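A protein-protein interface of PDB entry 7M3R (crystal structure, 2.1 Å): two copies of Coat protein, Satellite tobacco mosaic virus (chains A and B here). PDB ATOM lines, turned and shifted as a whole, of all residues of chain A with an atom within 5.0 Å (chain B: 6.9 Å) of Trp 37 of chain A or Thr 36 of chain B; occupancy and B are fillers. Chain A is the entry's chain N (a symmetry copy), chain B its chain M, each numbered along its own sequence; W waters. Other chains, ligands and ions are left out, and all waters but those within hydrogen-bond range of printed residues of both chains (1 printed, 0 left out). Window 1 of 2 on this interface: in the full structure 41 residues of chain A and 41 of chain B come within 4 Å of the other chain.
Of the 13 printed residues of chain B, 8 touch a printed residue of chain A.
Printed residues of chain B that touch a printed residue of chain A: Pro 33, Thr 34, Pro 35, Thr 36, Trp 37, Arg 66, Ser 69 and Phe 70.
Hydrophobic or aromatic side chains of chain B that line the printed part of chain A: Pro 33, Pro 35, Trp 37 and Phe 70.
Of the 12 printed residues of chain A, 7 touch a printed residue of chain B.
Printed residues of chain A that touch a printed residue of chain B: Pro 35, Thr 36, Trp 37, Arg 39, Phe 65, Arg 66 and Phe 70.
Along chain A the printed residues that touch a printed residue of chain B span positions 35 to 70.
Among the printed residues, 12 pairs touch across the chains.
Among the printed residues, no Asp or Glu carboxylate lies within 4 Å of a Lys or Arg side-chain nitrogen of the other chain.
Among the printed residues, merely in contact across the chains: Thr 36 of chain A with Trp 37 of chain B, Trp 37 of chain A with Thr 36 of chain B, Trp 37 of chain A with Trp 37 of chain B, Arg 39 of chain A with Pro 35 of chain B, Arg 66 of chain A with Phe 70 of chain B and Phe 70 of chain A with Arg 66 of chain B.
Pro 35 of chain A touches Arg 66 of chain B, and with the chains exchanged Arg 66 of chain A touches Pro 35 of chain B.
Thr 36 of chain A touches Trp 37 of chain B, and with the chains exchanged Trp 37 of chain A touches Thr 36 of chain B.
Trp 37 of chain A touches its own counterpart, Trp 37 of chain B.
Arg 66 of chain A touches Phe 70 of chain B, and with the chains exchanged Phe 70 of chain A touches Arg 66 of chain B.
Positions printed for both chains: 35, 36, 37, 38, 66, 70, 157 and 158.
The backbone NH (N) of Phe 158 of chain B sits at hydrogen-bond distance from the backbone carbonyl oxygen (O) of Trp 37 of chain B (2.9 Å).
O of Trp 37 of chain A lies within hydrogen-bond range of N of Phe 158 of chain A (2.7 Å).
The backbone NH (N) of Arg 39 of chain A is in hydrogen-bond range of the backbone carbonyl oxygen (O) of Cys 156 of chain A, 2.9 Å away.
The backbone carbonyl oxygen (O) of Phe 65 of chain A lies within hydrogen-bond range of the guanidinium group (NH1) of Arg 39 of chain A (2.7 Å).
The side-chain amide oxygen of Asn 32 of chain B sits close to the backbone NH of Thr 34 of chain B, at 3.2 Å.
Of chain B, only Thr 36 (3.6 Å) and Trp 37 (3.4 Å) come within 4 Å of Trp 37 of chain A.
Thr 36 of chain B touches one residue of chain A.
Of the printed residues of chain A, Pro 33 of chain B touches Arg 39 and Phe 65.
Of the printed residues of chain B, Pro 35 of chain A touches Arg 66 (2.9 Å).
The nearest residue of chain B that does not touch Trp 37 of chain A is Pro 35 of chain B (4.2 Å).
Water W1 lies within hydrogen-bond range of NH2 of Arg 39 of chain A (2.7 Å) and O of Asn 32 of chain B (2.9 Å).
The backbone carbonyl oxygen of Pro 35 of chain B lies within hydrogen-bond range of the guanidinium group of Arg 66 of chain A.
O of Ser 69 of chain B sits at hydrogen-bond distance from NH1 of Arg 66 of chain A (3.2 Å).
O of Pro 33 of chain B lies close to O of Phe 65 of chain A (3.4 Å).
The backbone carbonyl oxygen (O) of Pro 33 of chain B is in hydrogen-bond range of the guanidinium group (NH2) of Arg 39 of chain A, 2.7 Å away.
NH2 of Arg 66 of chain A sits at hydrogen-bond distance from O of Thr 34 of chain B, at 3.1 Å.
The guanidinium group of Arg 66 of chain B sits at hydrogen-bond distance from the backbone carbonyl oxygen of Pro 35 of chain A (2.9 Å).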
ATOM      1  N   PRO A  35      -5.457  -5.360  -1.219  1.00  0.00           N
ATOM      2  CA  PRO A  35      -5.337  -4.188  -2.100  1.00  0.00           C
ATOM      3  C   PRO A  35      -6.285  -4.218  -3.290  1.00  0.00           C
ATOM      4  O   PRO A  35      -7.020  -5.191  -3.494  1.00  0.00           O
ATOM      5  CB  PRO A  35      -3.873  -4.251  -2.556  1.00  0.00           C
ATOM      6  CG  PRO A  35      -3.577  -5.733  -2.589  1.00  0.00           C
ATOM      7  CD  PRO A  35      -4.393  -6.353  -1.466  1.00  0.00           C
ATOM      8  N   THR A  36      -6.276  -3.144  -4.080  1.00  0.00           N
ATOM      9  CA  THR A  36      -7.086  -3.070  -5.284  1.00  0.00           C
ATOM     10  C   THR A  36      -6.414  -3.830  -6.426  1.00  0.00           C
ATOM     11  O   THR A  36      -5.252  -4.236  -6.342  1.00  0.00           O
ATOM     12  CB  THR A  36      -7.321  -1.615  -5.690  1.00  0.00           C
ATOM     13  OG1 THR A  36      -6.062  -0.967  -5.901  1.00  0.00           O
ATOM     14  CG2 THR A  36      -8.097  -0.871  -4.609  1.00  0.00           C
ATOM     15  N   TRP A  37      -7.158  -4.015  -7.515  1.00  0.00           N
ATOM     16  CA  TRP A  37      -6.668  -4.803  -8.642  1.00  0.00           C
ATOM     17  C   TRP A  37      -7.321  -4.305  -9.921  1.00  0.00           C
ATOM     18  O   TRP A  37      -8.550  -4.329 -10.041  1.00  0.00           O
ATOM     19  CB  TRP A  37      -6.962  -6.292  -8.432  1.00  0.00           C
ATOM     20  CG  TRP A  37      -5.974  -7.227  -9.065  1.00  0.00           C
ATOM     21  CD1 TRP A  37      -4.886  -6.893  -9.821  1.00  0.00           C
ATOM     22  CD2 TRP A  37      -5.986  -8.657  -8.990  1.00  0.00           C
ATOM     23  NE1 TRP A  37      -4.223  -8.027 -10.220  1.00  0.00           N
ATOM     24  CE2 TRP A  37      -4.877  -9.123  -9.724  1.00  0.00           C
ATOM     25  CE3 TRP A  37      -6.826  -9.590  -8.375  1.00  0.00           C
ATOM     26  CZ2 TRP A  37      -4.589 -10.478  -9.858  1.00  0.00           C
ATOM     27  CZ3 TRP A  37      -6.538 -10.934  -8.512  1.00  0.00           C
ATOM     28  CH2 TRP A  37      -5.429 -11.366  -9.247  1.00  0.00           C
ATOM     29  N   VAL A  38      -6.501  -3.852 -10.862  1.00  0.00           N
ATOM     30  CA  VAL A  38      -6.962  -3.471 -12.192  1.00  0.00           C
ATOM     31  C   VAL A  38      -6.926  -4.711 -13.074  1.00  0.00           C
ATOM     32  O   VAL A  38      -5.896  -5.390 -13.165  1.00  0.00           O
ATOM     33  CB  VAL A  38      -6.089  -2.350 -12.778  1.00  0.00           C
ATOM     34  CG1 VAL A  38      -6.579  -1.976 -14.167  1.00  0.00           C
ATOM     35  CG2 VAL A  38      -6.096  -1.143 -11.859  1.00  0.00           C
ATOM     36  N   ARG A  39      -8.049  -5.008 -13.728  1.00  0.00           N
ATOM     37  CA  ARG A  39      -8.221  -6.295 -14.383  1.00  0.00           C
ATOM     38  C   ARG A  39      -8.977  -6.144 -15.695  1.00  0.00           C
ATOM     39  O   ARG A  39      -9.656  -5.143 -15.940  1.00  0.00           O
ATOM     40  CB  ARG A  39      -8.981  -7.275 -13.474  1.00  0.00           C
ATOM     41  CG  ARG A  39      -8.249  -7.660 -12.203  1.00  0.00           C
ATOM     42  CD  ARG A  39      -7.083  -8.585 -12.511  1.00  0.00           C
ATOM     43  NE  ARG A  39      -7.519  -9.792 -13.201  1.00  0.00           N
ATOM     44  CZ  ARG A  39      -8.093 -10.826 -12.604  1.00  0.00           C
ATOM     45  NH1 ARG A  39      -8.326 -10.829 -11.302  1.00  0.00           N
ATOM     46  NH2 ARG A  39      -8.443 -11.882 -13.332  1.00  0.00           N
ATOM     47  N   PHE A  65     -12.077 -15.785 -11.488  1.00  0.00           N
ATOM     48  CA  PHE A  65     -11.307 -14.602 -11.837  1.00  0.00           C
ATOM     49  C   PHE A  65     -10.391 -14.131 -10.716  1.00  0.00           C
ATOM     50  O   PHE A  65      -9.703 -13.118 -10.883  1.00  0.00           O
ATOM     51  CB  PHE A  65     -12.254 -13.459 -12.225  1.00  0.00           C
ATOM     52  CG  PHE A  65     -13.253 -13.837 -13.278  1.00  0.00           C
ATOM     53  CD1 PHE A  65     -12.843 -14.440 -14.456  1.00  0.00           C
ATOM     54  CD2 PHE A  65     -14.604 -13.597 -13.087  1.00  0.00           C
ATOM     55  CE1 PHE A  65     -13.759 -14.792 -15.426  1.00  0.00           C
ATOM     56  CE2 PHE A  65     -15.527 -13.946 -14.057  1.00  0.00           C
ATOM     57  CZ  PHE A  65     -15.104 -14.543 -15.225  1.00  0.00           C
ATOM     58  N   ARG A  66     -10.357 -14.839  -9.587  1.00  0.00           N
ATOM     59  CA  ARG A  66      -9.589 -14.440  -8.413  1.00  0.00           C
ATOM     60  C   ARG A  66     -10.148 -13.172  -7.772  1.00  0.00           C
ATOM     61  O   ARG A  66      -9.396 -12.367  -7.217  1.00  0.00           O
ATOM     62  CB  ARG A  66      -8.109 -14.234  -8.749  1.00  0.00           C
ATOM     63  CG  ARG A  66      -7.424 -15.395  -9.447  1.00  0.00           C
ATOM     64  CD  ARG A  66      -5.923 -15.306  -9.221  1.00  0.00           C
ATOM     65  NE  ARG A  66      -5.137 -16.078 -10.176  1.00  0.00           N
ATOM     66  CZ  ARG A  66      -4.849 -17.367 -10.047  1.00  0.00           C
ATOM     67  NH1 ARG A  66      -5.339 -18.091  -9.055  1.00  0.00           N
ATOM     68  NH2 ARG A  66      -4.045 -17.943 -10.935  1.00  0.00           N
ATOM     69  N   THR A  67     -11.470 -12.985  -7.838  1.00  0.00           N
ATOM     70  CA  THR A  67     -12.096 -11.755  -7.368  1.00  0.00           C
ATOM     71  C   THR A  67     -13.288 -12.020  -6.454  1.00  0.00           C
ATOM     72  O   THR A  67     -14.160 -11.156  -6.324  1.00  0.00           O
ATOM     73  CB  THR A  67     -12.541 -10.894  -8.554  1.00  0.00           C
ATOM     74  OG1 THR A  67     -13.504 -11.613  -9.334  1.00  0.00           O
ATOM     75  CG2 THR A  67     -11.353 -10.524  -9.432  1.00  0.00           C
ATOM     76  N   PHE A  70     -13.812  -9.510  -3.486  1.00  0.00           N
ATOM     77  CA  PHE A  70     -14.316  -8.172  -3.746  1.00  0.00           C
ATOM     78  C   PHE A  70     -15.839  -8.164  -3.740  1.00  0.00           C
ATOM     79  O   PHE A  70     -16.490  -9.151  -4.096  1.00  0.00           O
ATOM     80  CB  PHE A  70     -13.816  -7.649  -5.095  1.00  0.00           C
ATOM     81  CG  PHE A  70     -12.327  -7.467  -5.172  1.00  0.00           C
ATOM     82  CD1 PHE A  70     -11.724  -6.347  -4.630  1.00  0.00           C
ATOM     83  CD2 PHE A  70     -11.532  -8.408  -5.809  1.00  0.00           C
ATOM     84  CE1 PHE A  70     -10.354  -6.171  -4.711  1.00  0.00           C
ATOM     85  CE2 PHE A  70     -10.161  -8.239  -5.891  1.00  0.00           C
ATOM     86  CZ  PHE A  70      -9.572  -7.117  -5.343  1.00  0.00           C
ATOM     87  N   CYS A 156     -11.785  -3.141 -15.660  1.00  0.00           N
ATOM     88  CA  CYS A 156     -12.337  -2.556 -14.449  1.00  0.00           C
ATOM     89  C   CYS A 156     -11.289  -2.560 -13.345  1.00  0.00           C
ATOM     90  O   CYS A 156     -10.229  -3.178 -13.461  1.00  0.00           O
ATOM     91  CB  CYS A 156     -13.592  -3.313 -14.004  1.00  0.00           C
ATOM     92  SG  CYS A 156     -13.400  -5.117 -13.998  1.00  0.00           S
ATOM     93  N   CYS A 157     -11.606  -1.847 -12.265  1.00  0.00           N
ATOM     94  CA  CYS A 157     -10.755  -1.752 -11.087  1.00  0.00           C
ATOM     95  C   CYS A 157     -11.496  -2.356  -9.904  1.00  0.00           C
ATOM     96  O   CYS A 157     -12.549  -1.846  -9.502  1.00  0.00           O
ATOM     97  CB  CYS A 157     -10.387  -0.300 -10.782  1.00  0.00           C
ATOM     98  SG  CYS A 157      -9.428   0.532 -12.050  1.00  0.00           S
ATOM     99  N   PHE A 158     -10.950  -3.430  -9.348  1.00  0.00           N
ATOM    100  CA  PHE A 158     -11.539  -4.073  -8.184  1.00  0.00           C
ATOM    101  C   PHE A 158     -11.038  -3.410  -6.909  1.00  0.00           C
ATOM    102  O   PHE A 158      -9.856  -3.077  -6.787  1.00  0.00           O
ATOM    103  CB  PHE A 158     -11.212  -5.566  -8.174  1.00  0.00           C
ATOM    104  CG  PHE A 158     -11.994  -6.360  -9.182  1.00  0.00           C
ATOM    105  CD1 PHE A 158     -13.226  -6.900  -8.852  1.00  0.00           C
ATOM    106  CD2 PHE A 158     -11.500  -6.567 -10.458  1.00  0.00           C
ATOM    107  CE1 PHE A 158     -13.948  -7.630  -9.776  1.00  0.00           C
ATOM    108  CE2 PHE A 158     -12.219  -7.303 -11.386  1.00  0.00           C
ATOM    109  CZ  PHE A 158     -13.445  -7.831 -11.042  1.00  0.00           C
ATOM    110  N   ASN B  32      -6.782 -14.336 -19.980  1.00  0.00           N
ATOM    111  CA  ASN B  32      -6.373 -15.199 -18.880  1.00  0.00           C
ATOM    112  C   ASN B  32      -7.144 -14.769 -17.637  1.00  0.00           C
ATOM    113  O   ASN B  32      -6.780 -13.774 -16.998  1.00  0.00           O
ATOM    114  CB  ASN B  32      -4.866 -15.114 -18.645  1.00  0.00           C
ATOM    115  CG  ASN B  32      -4.410 -15.992 -17.501  1.00  0.00           C
ATOM    116  OD1 ASN B  32      -5.160 -16.840 -17.018  1.00  0.00           O
ATOM    117  ND2 ASN B  32      -3.173 -15.796 -17.062  1.00  0.00           N
ATOM    118  N   PRO B  33      -8.218 -15.472 -17.267  1.00  0.00           N
ATOM    119  CA  PRO B  33      -9.019 -15.018 -16.118  1.00  0.00           C
ATOM    120  C   PRO B  33      -8.293 -15.126 -14.792  1.00  0.00           C
ATOM    121  O   PRO B  33      -8.724 -14.498 -13.817  1.00  0.00           O
ATOM    122  CB  PRO B  33     -10.249 -15.937 -16.158  1.00  0.00           C
ATOM    123  CG  PRO B  33      -9.757 -17.189 -16.832  1.00  0.00           C
ATOM    124  CD  PRO B  33      -8.743 -16.720 -17.852  1.00  0.00           C
ATOM    125  N   THR B  34      -7.205 -15.889 -14.724  1.00  0.00           N
ATOM    126  CA  THR B  34      -6.509 -16.186 -13.473  1.00  0.00           C
ATOM    127  C   THR B  34      -5.033 -15.859 -13.649  1.00  0.00           C
ATOM    128  O   THR B  34      -4.198 -16.759 -13.799  1.00  0.00           O
ATOM    129  CB  THR B  34      -6.710 -17.649 -13.076  1.00  0.00           C
ATOM    130  OG1 THR B  34      -6.492 -18.488 -14.218  1.00  0.00           O
ATOM    131  CG2 THR B  34      -8.125 -17.873 -12.554  1.00  0.00           C
ATOM    132  N   PRO B  35      -4.676 -14.582 -13.633  1.00  0.00           N
ATOM    133  CA  PRO B  35      -3.282 -14.184 -13.854  1.00  0.00           C
ATOM    134  C   PRO B  35      -2.462 -14.283 -12.570  1.00  0.00           C
ATOM    135  O   PRO B  35      -2.953 -14.656 -11.506  1.00  0.00           O
ATOM    136  CB  PRO B  35      -3.410 -12.736 -14.330  1.00  0.00           C
ATOM    137  CG  PRO B  35      -4.640 -12.229 -13.624  1.00  0.00           C
ATOM    138  CD  PRO B  35      -5.576 -13.418 -13.512  1.00  0.00           C
ATOM    139  N   THR B  36      -1.181 -13.943 -12.696  1.00  0.00           N
ATOM    140  CA  THR B  36      -0.289 -13.876 -11.552  1.00  0.00           C
ATOM    141  C   THR B  36      -0.568 -12.603 -10.753  1.00  0.00           C
ATOM    142  O   THR B  36      -1.442 -11.801 -11.097  1.00  0.00           O
ATOM    143  CB  THR B  36       1.169 -13.929 -12.007  1.00  0.00           C
ATOM    144  OG1 THR B  36       1.464 -12.790 -12.826  1.00  0.00           O
ATOM    145  CG2 THR B  36       1.440 -15.202 -12.793  1.00  0.00           C
ATOM    146  N   TRP B  37       0.188 -12.405  -9.674  1.00  0.00           N
ATOM    147  CA  TRP B  37      -0.005 -11.232  -8.825  1.00  0.00           C
ATOM    148  C   TRP B  37       1.219 -11.061  -7.941  1.00  0.00           C
ATOM    149  O   TRP B  37       1.547 -11.958  -7.158  1.00  0.00           O
ATOM    150  CB  TRP B  37      -1.270 -11.381  -7.979  1.00  0.00           C
ATOM    151  CG  TRP B  37      -1.856 -10.076  -7.516  1.00  0.00           C
ATOM    152  CD1 TRP B  37      -1.358  -8.824  -7.739  1.00  0.00           C
ATOM    153  CD2 TRP B  37      -3.058  -9.897  -6.754  1.00  0.00           C
ATOM    154  NE1 TRP B  37      -2.174  -7.881  -7.168  1.00  0.00           N
ATOM    155  CE2 TRP B  37      -3.223  -8.513  -6.556  1.00  0.00           C
ATOM    156  CE3 TRP B  37      -4.009 -10.775  -6.222  1.00  0.00           C
ATOM    157  CZ2 TRP B  37      -4.302  -7.983  -5.846  1.00  0.00           C
ATOM    158  CZ3 TRP B  37      -5.078 -10.248  -5.517  1.00  0.00           C
ATOM    159  CH2 TRP B  37      -5.216  -8.865  -5.337  1.00  0.00           C
ATOM    160  N   VAL B  38       1.890  -9.923  -8.065  1.00  0.00           N
ATOM    161  CA  VAL B  38       3.009  -9.577  -7.198  1.00  0.00           C
ATOM    162  C   VAL B  38       2.457  -8.893  -5.955  1.00  0.00           C
ATOM    163  O   VAL B  38       1.638  -7.971  -6.055  1.00  0.00           O
ATOM    164  CB  VAL B  38       4.017  -8.676  -7.928  1.00  0.00           C
ATOM    165  CG1 VAL B  38       5.020  -8.096  -6.940  1.00  0.00           C
ATOM    166  CG2 VAL B  38       4.724  -9.460  -9.022  1.00  0.00           C
ATOM    167  N   ARG B  66      -6.570 -12.107  -0.339  1.00  0.00           N
ATOM    168  CA  ARG B  66      -7.098 -12.236  -1.690  1.00  0.00           C
ATOM    169  C   ARG B  66      -6.311 -13.251  -2.515  1.00  0.00           C
ATOM    170  O   ARG B  66      -6.273 -13.161  -3.745  1.00  0.00           O
ATOM    171  CB  ARG B  66      -7.113 -10.889  -2.419  1.00  0.00           C
ATOM    172  CG  ARG B  66      -7.749  -9.723  -1.670  1.00  0.00           C
ATOM    173  CD  ARG B  66      -8.063  -8.598  -2.657  1.00  0.00           C
ATOM    174  NE  ARG B  66      -8.412  -7.333  -2.019  1.00  0.00           N
ATOM    175  CZ  ARG B  66      -9.643  -6.970  -1.692  1.00  0.00           C
ATOM    176  NH1 ARG B  66     -10.672  -7.778  -1.868  1.00  0.00           N
ATOM    177  NH2 ARG B  66      -9.849  -5.761  -1.178  1.00  0.00           N
ATOM    178  N   SER B  69      -7.046 -18.320  -3.980  1.00  0.00           N
ATOM    179  CA  SER B  69      -7.181 -18.960  -5.281  1.00  0.00           C
ATOM    180  C   SER B  69      -5.868 -19.533  -5.796  1.00  0.00           C
ATOM    181  O   SER B  69      -5.879 -20.268  -6.791  1.00  0.00           O
ATOM    182  CB  SER B  69      -7.729 -17.957  -6.301  1.00  0.00           C
ATOM    183  OG  SER B  69      -6.868 -16.836  -6.418  1.00  0.00           O
ATOM    184  N   PHE B  70      -4.746 -19.212  -5.159  1.00  0.00           N
ATOM    185  CA  PHE B  70      -3.442 -19.703  -5.574  1.00  0.00           C
ATOM    186  C   PHE B  70      -3.062 -20.945  -4.779  1.00  0.00           C
ATOM    187  O   PHE B  70      -3.553 -21.182  -3.672  1.00  0.00           O
ATOM    188  CB  PHE B  70      -2.370 -18.625  -5.390  1.00  0.00           C
ATOM    189  CG  PHE B  70      -2.476 -17.481  -6.359  1.00  0.00           C
ATOM    190  CD1 PHE B  70      -1.873 -17.552  -7.604  1.00  0.00           C
ATOM    191  CD2 PHE B  70      -3.161 -16.325  -6.018  1.00  0.00           C
ATOM    192  CE1 PHE B  70      -1.960 -16.497  -8.495  1.00  0.00           C
ATOM    193  CE2 PHE B  70      -3.253 -15.270  -6.905  1.00  0.00           C
ATOM    194  CZ  PHE B  70      -2.652 -15.357  -8.144  1.00  0.00           C
ATOM    195  N   CYS B 157       5.619 -13.643  -5.691  1.00  0.00           N
ATOM    196  CA  CYS B 157       4.910 -13.654  -6.968  1.00  0.00           C
ATOM    197  C   CYS B 157       3.922 -14.817  -6.947  1.00  0.00           C
ATOM    198  O   CYS B 157       4.304 -15.961  -7.215  1.00  0.00           O
ATOM    199  CB  CYS B 157       5.879 -13.791  -8.141  1.00  0.00           C
ATOM    200  SG  CYS B 157       7.250 -12.621  -8.173  1.00  0.00           S
ATOM    201  N   PHE B 158       2.660 -14.531  -6.631  1.00  0.00           N
ATOM    202  CA  PHE B 158       1.629 -15.559  -6.670  1.00  0.00           C
ATOM    203  C   PHE B 158       1.356 -15.970  -8.112  1.00  0.00           C
ATOM    204  O   PHE B 158       1.107 -15.121  -8.975  1.00  0.00           O
ATOM    205  CB  PHE B 158       0.346 -15.053  -6.013  1.00  0.00           C
ATOM    206  CG  PHE B 158       0.411 -14.996  -4.513  1.00  0.00           C
ATOM    207  CD1 PHE B 158       0.104 -16.112  -3.751  1.00  0.00           C
ATOM    208  CD2 PHE B 158       0.768 -13.824  -3.862  1.00  0.00           C
ATOM    209  CE1 PHE B 158       0.159 -16.066  -2.369  1.00  0.00           C
ATOM    210  CE2 PHE B 158       0.824 -13.771  -2.482  1.00  0.00           C
ATOM    211  CZ  PHE B 158       0.519 -14.896  -1.734  1.00  0.00           C
ATOM    212  N   ASN B 159       1.404 -17.274  -8.375  1.00  0.00           N
ATOM    213  CA  ASN B 159       1.176 -17.790  -9.722  1.00  0.00           C
ATOM    214  C   ASN B 159       0.488 -19.151  -9.680  1.00  0.00           C
ATOM    215  O   ASN B 159      -0.247 -19.519 -10.595  1.00  0.00           O
ATOM    216  CB  ASN B 159       2.500 -17.886 -10.488  1.00  0.00           C
ATOM    217  CG  ASN B 159       3.451 -18.908  -9.891  1.00  0.00           C
ATOM    218  OD1 ASN B 159       3.476 -20.064 -10.310  1.00  0.00           O
ATOM    219  ND2 ASN B 159       4.239 -18.483  -8.911  1.00  0.00           N
ATOM    220  OXT ASN B 159       0.636 -19.917  -8.728  1.00  0.00           O
HETATM  221  O   HOH W   1      -8.493 -11.671 -16.073  1.00  0.00           O
